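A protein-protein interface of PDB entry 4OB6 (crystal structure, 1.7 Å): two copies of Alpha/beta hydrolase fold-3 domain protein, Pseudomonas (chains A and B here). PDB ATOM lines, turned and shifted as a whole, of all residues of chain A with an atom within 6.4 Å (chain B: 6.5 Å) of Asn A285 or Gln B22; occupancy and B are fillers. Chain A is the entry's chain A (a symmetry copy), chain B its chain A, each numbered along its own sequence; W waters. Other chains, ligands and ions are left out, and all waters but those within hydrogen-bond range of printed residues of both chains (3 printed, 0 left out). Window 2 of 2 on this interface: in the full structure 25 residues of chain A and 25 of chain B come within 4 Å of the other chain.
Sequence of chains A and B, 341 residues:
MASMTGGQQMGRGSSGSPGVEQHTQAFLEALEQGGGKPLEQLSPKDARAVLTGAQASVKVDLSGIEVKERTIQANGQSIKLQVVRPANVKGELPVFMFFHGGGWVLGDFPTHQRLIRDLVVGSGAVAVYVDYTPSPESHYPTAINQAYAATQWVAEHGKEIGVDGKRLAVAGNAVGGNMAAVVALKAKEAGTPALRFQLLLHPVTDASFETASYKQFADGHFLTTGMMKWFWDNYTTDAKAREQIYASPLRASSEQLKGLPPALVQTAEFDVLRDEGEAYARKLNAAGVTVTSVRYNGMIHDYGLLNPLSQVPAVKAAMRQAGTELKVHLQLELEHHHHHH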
ATOM      1  N   TYR A 280      -3.137  32.014  -8.910  1.00  0.00           N
ATOM      2  CA  TYR A 280      -3.052  30.676  -8.336  1.00  0.00           C
ATOM      3  C   TYR A 280      -2.753  29.658  -9.437  1.00  0.00           C
ATOM      4  O   TYR A 280      -1.950  28.735  -9.247  1.00  0.00           O
ATOM      5  CB  TYR A 280      -4.340  30.316  -7.589  1.00  0.00           C
ATOM      6  CG  TYR A 280      -4.235  29.006  -6.830  1.00  0.00           C
ATOM      7  CD1 TYR A 280      -3.296  28.855  -5.817  1.00  0.00           C
ATOM      8  CD2 TYR A 280      -5.062  27.932  -7.130  1.00  0.00           C
ATOM      9  CE1 TYR A 280      -3.186  27.670  -5.109  1.00  0.00           C
ATOM     10  CE2 TYR A 280      -4.960  26.737  -6.431  1.00  0.00           C
ATOM     11  CZ  TYR A 280      -4.021  26.621  -5.419  1.00  0.00           C
ATOM     12  OH  TYR A 280      -3.890  25.451  -4.716  1.00  0.00           O
ATOM     13  N   ALA A 281      -3.393  29.826 -10.594  1.00  0.00           N
ATOM     14  CA  ALA A 281      -3.092  28.980 -11.739  1.00  0.00           C
ATOM     15  C   ALA A 281      -1.605  29.061 -12.108  1.00  0.00           C
ATOM     16  O   ALA A 281      -0.982  28.040 -12.420  1.00  0.00           O
ATOM     17  CB  ALA A 281      -3.975  29.362 -12.946  1.00  0.00           C
ATOM     18  N   ARG A 282      -1.027  30.257 -12.054  1.00  0.00           N
ATOM     19  CA  ARG A 282       0.392  30.397 -12.378  1.00  0.00           C
ATOM     20  C   ARG A 282       1.257  29.663 -11.373  1.00  0.00           C
ATOM     21  O   ARG A 282       2.247  29.022 -11.742  1.00  0.00           O
ATOM     22  CB  ARG A 282       0.818  31.861 -12.423  1.00  0.00           C
ATOM     23  CG  ARG A 282       0.355  32.599 -13.665  1.00  0.00           C
ATOM     24  CD  ARG A 282       1.099  33.914 -13.734  1.00  0.00           C
ATOM     25  NE  ARG A 282       0.768  34.670 -14.934  1.00  0.00           N
ATOM     26  CZ  ARG A 282       1.296  35.858 -15.222  1.00  0.00           C
ATOM     27  NH1 ARG A 282       2.169  36.415 -14.392  1.00  0.00           N
ATOM     28  NH2 ARG A 282       0.952  36.489 -16.334  1.00  0.00           N
ATOM     29  N   LYS A 283       0.890  29.758 -10.100  1.00  0.00           N
ATOM     30  CA  LYS A 283       1.672  29.080  -9.068  1.00  0.00           C
ATOM     31  C   LYS A 283       1.580  27.570  -9.229  1.00  0.00           C
ATOM     32  O   LYS A 283       2.567  26.861  -9.031  1.00  0.00           O
ATOM     33  CB  LYS A 283       1.236  29.518  -7.669  1.00  0.00           C
ATOM     34  CG  LYS A 283       1.662  30.941  -7.352  1.00  0.00           C
ATOM     35  CD  LYS A 283       1.334  31.307  -5.919  1.00  0.00           C
ATOM     36  CE  LYS A 283       1.700  32.767  -5.619  1.00  0.00           C
ATOM     37  NZ  LYS A 283       3.158  32.925  -5.360  1.00  0.00           N
ATOM     38  N   LEU A 284       0.404  27.070  -9.593  1.00  0.00           N
ATOM     39  CA  LEU A 284       0.270  25.642  -9.833  1.00  0.00           C
ATOM     40  C   LEU A 284       1.193  25.219 -10.975  1.00  0.00           C
ATOM     41  O   LEU A 284       1.925  24.226 -10.874  1.00  0.00           O
ATOM     42  CB  LEU A 284      -1.178  25.288 -10.157  1.00  0.00           C
ATOM     43  CG  LEU A 284      -2.186  25.412  -9.017  1.00  0.00           C
ATOM     44  CD1 LEU A 284      -3.587  25.176  -9.554  1.00  0.00           C
ATOM     45  CD2 LEU A 284      -1.877  24.396  -7.909  1.00  0.00           C
ATOM     46  N   ASN A 285       1.172  25.986 -12.064  1.00  0.00           N
ATOM     47  CA  ASN A 285       2.019  25.681 -13.209  1.00  0.00           C
ATOM     48  C   ASN A 285       3.500  25.694 -12.841  1.00  0.00           C
ATOM     49  O   ASN A 285       4.257  24.817 -13.273  1.00  0.00           O
ATOM     50  CB  ASN A 285       1.732  26.657 -14.356  1.00  0.00           C
ATOM     51  CG  ASN A 285       2.664  26.466 -15.528  1.00  0.00           C
ATOM     52  OD1 ASN A 285       2.563  25.474 -16.256  1.00  0.00           O
ATOM     53  ND2 ASN A 285       3.572  27.423 -15.729  1.00  0.00           N
ATOM     54  N   ALA A 286       3.906  26.673 -12.033  1.00  0.00           N
ATOM     55  CA  ALA A 286       5.313  26.801 -11.654  1.00  0.00           C
ATOM     56  C   ALA A 286       5.734  25.614 -10.803  1.00  0.00           C
ATOM     57  O   ALA A 286       6.917  25.269 -10.741  1.00  0.00           O
ATOM     58  CB  ALA A 286       5.567  28.108 -10.913  1.00  0.00           C
ATOM     59  N   ALA A 287       4.761  24.990 -10.151  1.00  0.00           N
ATOM     60  CA  ALA A 287       5.025  23.847  -9.288  1.00  0.00           C
ATOM     61  C   ALA A 287       4.916  22.533 -10.046  1.00  0.00           C
ATOM     62  O   ALA A 287       4.998  21.459  -9.448  1.00  0.00           O
ATOM     63  CB  ALA A 287       4.082  23.855  -8.089  1.00  0.00           C
ATOM     64  N   GLY A 288       4.720  22.614 -11.361  1.00  0.00           N
ATOM     65  CA  GLY A 288       4.683  21.427 -12.194  1.00  0.00           C
ATOM     66  C   GLY A 288       3.331  20.762 -12.301  1.00  0.00           C
ATOM     67  O   GLY A 288       3.206  19.690 -12.900  1.00  0.00           O
ATOM     68  N   VAL A 289       2.314  21.384 -11.714  1.00  0.00           N
ATOM     69  CA  VAL A 289       0.952  20.886 -11.809  1.00  0.00           C
ATOM     70  C   VAL A 289       0.407  21.217 -13.191  1.00  0.00           C
ATOM     71  O   VAL A 289       0.700  22.283 -13.725  1.00  0.00           O
ATOM     72  CB  VAL A 289       0.063  21.540 -10.725  1.00  0.00           C
ATOM     73  CG1 VAL A 289      -1.388  21.101 -10.863  1.00  0.00           C
ATOM     74  CG2 VAL A 289       0.596  21.190  -9.334  1.00  0.00           C
ATOM     75  N   THR A 290      -0.350  20.293 -13.780  1.00  0.00           N
ATOM     76  CA  THR A 290      -0.995  20.533 -15.072  1.00  0.00           C
ATOM     77  C   THR A 290      -2.164  21.488 -14.877  1.00  0.00           C
ATOM     78  O   THR A 290      -3.071  21.202 -14.091  1.00  0.00           O
ATOM     79  CB  THR A 290      -1.503  19.222 -15.675  1.00  0.00           C
ATOM     80  OG1 THR A 290      -0.383  18.389 -16.019  1.00  0.00           O
ATOM     81  CG2 THR A 290      -2.344  19.486 -16.926  1.00  0.00           C
ATOM     82  N   VAL A 291      -2.138  22.621 -15.584  1.00  0.00           N
ATOM     83  CA  VAL A 291      -3.167  23.649 -15.418  1.00  0.00           C
ATOM     84  C   VAL A 291      -3.649  24.181 -16.757  1.00  0.00           C
ATOM     85  O   VAL A 291      -2.847  24.432 -17.665  1.00  0.00           O
ATOM     86  CB  VAL A 291      -2.634  24.866 -14.630  1.00  0.00           C
ATOM     87  CG1 VAL A 291      -3.751  25.873 -14.390  1.00  0.00           C
ATOM     88  CG2 VAL A 291      -2.066  24.440 -13.326  1.00  0.00           C
ATOM     89  N   GLY B  19       4.762  32.818 -15.946  1.00  0.00           N
ATOM     90  CA  GLY B  19       3.390  32.445 -16.191  1.00  0.00           C
ATOM     91  C   GLY B  19       3.191  31.654 -17.467  1.00  0.00           C
ATOM     92  O   GLY B  19       2.088  31.186 -17.725  1.00  0.00           O
ATOM     93  N   VAL B  20       4.241  31.500 -18.273  1.00  0.00           N
ATOM     94  CA  VAL B  20       4.118  30.655 -19.461  1.00  0.00           C
ATOM     95  C   VAL B  20       3.980  29.194 -19.036  1.00  0.00           C
ATOM     96  O   VAL B  20       4.739  28.707 -18.188  1.00  0.00           O
ATOM     97  CB  VAL B  20       5.309  30.837 -20.426  1.00  0.00           C
ATOM     98  CG1 VAL B  20       5.209  29.883 -21.623  1.00  0.00           C
ATOM     99  CG2 VAL B  20       5.361  32.273 -20.912  1.00  0.00           C
ATOM    100  N   GLU B  21       3.009  28.498 -19.620  1.00  0.00           N
ATOM    101  CA  GLU B  21       2.791  27.085 -19.315  1.00  0.00           C
ATOM    102  C   GLU B  21       4.087  26.288 -19.545  1.00  0.00           C
ATOM    103  O   GLU B  21       4.845  26.583 -20.477  1.00  0.00           O
ATOM    104  CB  GLU B  21       1.637  26.554 -20.170  1.00  0.00           C
ATOM    105  CG  GLU B  21       1.299  25.092 -19.955  1.00  0.00           C
ATOM    106  CD  GLU B  21       2.166  24.162 -20.773  1.00  0.00           C
ATOM    107  OE1 GLU B  21       2.563  24.552 -21.891  1.00  0.00           O
ATOM    108  OE2 GLU B  21       2.441  23.032 -20.305  1.00  0.00           O
ATOM    109  N   GLN B  22       4.334  25.292 -18.692  1.00  0.00           N
ATOM    110  CA  GLN B  22       5.646  24.621 -18.638  1.00  0.00           C
ATOM    111  C   GLN B  22       6.150  24.018 -19.956  1.00  0.00           C
ATOM    112  O   GLN B  22       7.307  24.235 -20.334  1.00  0.00           O
ATOM    113  CB  GLN B  22       5.693  23.589 -17.500  1.00  0.00           C
ATOM    114  CG  GLN B  22       4.608  22.523 -17.575  1.00  0.00           C
ATOM    115  CD  GLN B  22       4.655  21.546 -16.401  1.00  0.00           C
ATOM    116  OE1 GLN B  22       5.563  21.601 -15.564  1.00  0.00           O
ATOM    117  NE2 GLN B  22       3.677  20.649 -16.340  1.00  0.00           N
ATOM    118  N   HIS B  23       5.300  23.273 -20.659  1.00  0.00           N
ATOM    119  CA  HIS B  23       5.726  22.687 -21.926  1.00  0.00           C
ATOM    120  C   HIS B  23       5.977  23.765 -22.971  1.00  0.00           C
ATOM    121  O   HIS B  23       6.920  23.677 -23.769  1.00  0.00           O
ATOM    122  CB  HIS B  23       4.691  21.683 -22.421  1.00  0.00           C
ATOM    123  CG  HIS B  23       4.548  20.490 -21.528  1.00  0.00           C
ATOM    124  ND1 HIS B  23       5.472  19.464 -21.501  1.00  0.00           N
ATOM    125  CD2 HIS B  23       3.598  20.162 -20.622  1.00  0.00           C
ATOM    126  CE1 HIS B  23       5.093  18.557 -20.623  1.00  0.00           C
ATOM    127  NE2 HIS B  23       3.955  18.954 -20.075  1.00  0.00           N
ATOM    128  N   THR B  24       5.133  24.785 -22.963  1.00  0.00           N
ATOM    129  CA  THR B  24       5.298  25.905 -23.881  1.00  0.00           C
ATOM    130  C   THR B  24       6.612  26.631 -23.616  1.00  0.00           C
ATOM    131  O   THR B  24       7.319  27.017 -24.551  1.00  0.00           O
ATOM    132  CB  THR B  24       4.115  26.874 -23.753  1.00  0.00           C
ATOM    133  OG1 THR B  24       2.909  26.165 -24.070  1.00  0.00           O
ATOM    134  CG2 THR B  24       4.254  28.050 -24.709  1.00  0.00           C
ATOM    135  N   GLN B  25       6.941  26.817 -22.342  1.00  0.00           N
ATOM    136  CA  GLN B  25       8.191  27.496 -22.008  1.00  0.00           C
ATOM    137  C   GLN B  25       9.395  26.685 -22.490  1.00  0.00           C
ATOM    138  O   GLN B  25      10.360  27.251 -23.013  1.00  0.00           O
ATOM    139  CB  GLN B  25       8.277  27.750 -20.499  1.00  0.00           C
ATOM    140  CG  GLN B  25       9.586  28.397 -20.055  1.00  0.00           C
ATOM    141  CD  GLN B  25       9.811  29.763 -20.675  1.00  0.00           C
ATOM    142  OE1 GLN B  25       8.868  30.521 -20.914  1.00  0.00           O
ATOM    143  NE2 GLN B  25      11.074  30.089 -20.937  1.00  0.00           N
ATOM    144  N   ALA B  26       9.335  25.360 -22.324  1.00  0.00           N
ATOM    145  CA  ALA B  26      10.394  24.484 -22.837  1.00  0.00           C
ATOM    146  C   ALA B  26      10.522  24.602 -24.360  1.00  0.00           C
ATOM    147  O   ALA B  26      11.629  24.603 -24.902  1.00  0.00           O
ATOM    148  CB  ALA B  26      10.152  23.035 -22.419  1.00  0.00           C
ATOM    149  N   PHE B  27       9.389  24.700 -25.049  1.00  0.00           N
ATOM    150  CA  PHE B  27       9.379  24.909 -26.498  1.00  0.00           C
ATOM    151  C   PHE B  27      10.084  26.212 -26.873  1.00  0.00           C
ATOM    152  O   PHE B  27      10.918  26.237 -27.782  1.00  0.00           O
ATOM    153  CB  PHE B  27       7.926  24.888 -26.999  1.00  0.00           C
ATOM    154  CG  PHE B  27       7.744  25.334 -28.423  1.00  0.00           C
ATOM    155  CD1 PHE B  27       8.038  24.479 -29.473  1.00  0.00           C
ATOM    156  CD2 PHE B  27       7.235  26.596 -28.708  1.00  0.00           C
ATOM    157  CE1 PHE B  27       7.847  24.885 -30.793  1.00  0.00           C
ATOM    158  CE2 PHE B  27       7.046  27.009 -30.027  1.00  0.00           C
ATOM    159  CZ  PHE B  27       7.355  26.151 -31.065  1.00  0.00           C
ATOM    160  N   GLY B 298      -1.200  31.450 -20.103  1.00  0.00           N
ATOM    161  CA  GLY B 298      -0.031  30.593 -20.178  1.00  0.00           C
ATOM    162  C   GLY B 298       0.396  30.221 -21.586  1.00  0.00           C
ATOM    163  O   GLY B 298       1.450  29.620 -21.779  1.00  0.00           O
HETATM  164  O   HOH W   1       7.027  24.261 -14.259  1.00  0.00           O
HETATM  165  O   HOH W   2       1.348  19.366 -17.993  1.00  0.00           O
HETATM  166  O   HOH W   3      -0.052  32.859 -16.994  1.00  0.00           O
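Gly B19 touches Arg A282 (CA to NE, 3.7 Å).
CA of Glu B21 touches OD1 of Asn A285, 3.5 Å away.
Gly A288 touches Gln B22 (CA to OE1, 3.5 Å).
OE2 of Glu B21 lies within hydrogen-bond range of N of His B23, 2.9 Å away.
The side-chain hydroxyl of Thr B24 is in hydrogen-bond range of the side-chain carboxylate of Glu B21 (2.7 Å).
The backbone carbonyl oxygen of Gly B298 is in hydrogen-bond range of the backbone NH of Glu B21 (2.9 Å).
The backbone carbonyl oxygen (O) of Val B20 lies within hydrogen-bond range of the side-chain amide nitrogen (ND2) of Asn A285 (3.0 Å).
The side-chain amide oxygen (OD1) of Asn A285 lies within hydrogen-bond range of the backbone NH (N) of Gln B22 (3.0 Å).
Asn A285 touches just these residues of chain B: Val B20 (3.0 Å), Glu B21 (3.5 Å) and Gln B22 (3.0 Å).
Printed residues of chain B within 4 Å of Gly A288: Gln B22 (3.5 Å).
Of the printed residues of chain A, Gly B19 touches Arg A282 (3.7 Å).
Of the printed residues of chain A, Val B20 touches Asn A285 (3.0 Å).
Of the printed residues of chain A, Glu B21 touches Asn A285.
Gln B22 touches just these residues of chain A: Asn A285 (3.0 Å) and Gly A288 (3.5 Å).
No position is printed for both chains.
Of the 5 pairs that touch across the chains among the printed residues, none has its exchanged pair printed and touching as well.
Of the 10 printed residues of chain B, 4 touch a printed residue of chain A.
Printed residues of chain A that touch a printed residue of chain B: Arg A282, Asn A285 and Gly A288.
Among the printed residues, 5 pairs touch across the chains.
Water W2 lies within hydrogen-bond range of OG1 of Thr A290 (2.8 Å), NE2 of Gln B22 (3.1 Å) and NE2 of His B23 (3.4 Å).
Water W3 bridges O of Gly B19 and NE of Arg A282.
Water W1 lies within hydrogen-bond range of O of Asn A285 (3.0 Å) and OE1 of Gln B22 (3.3 Å).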
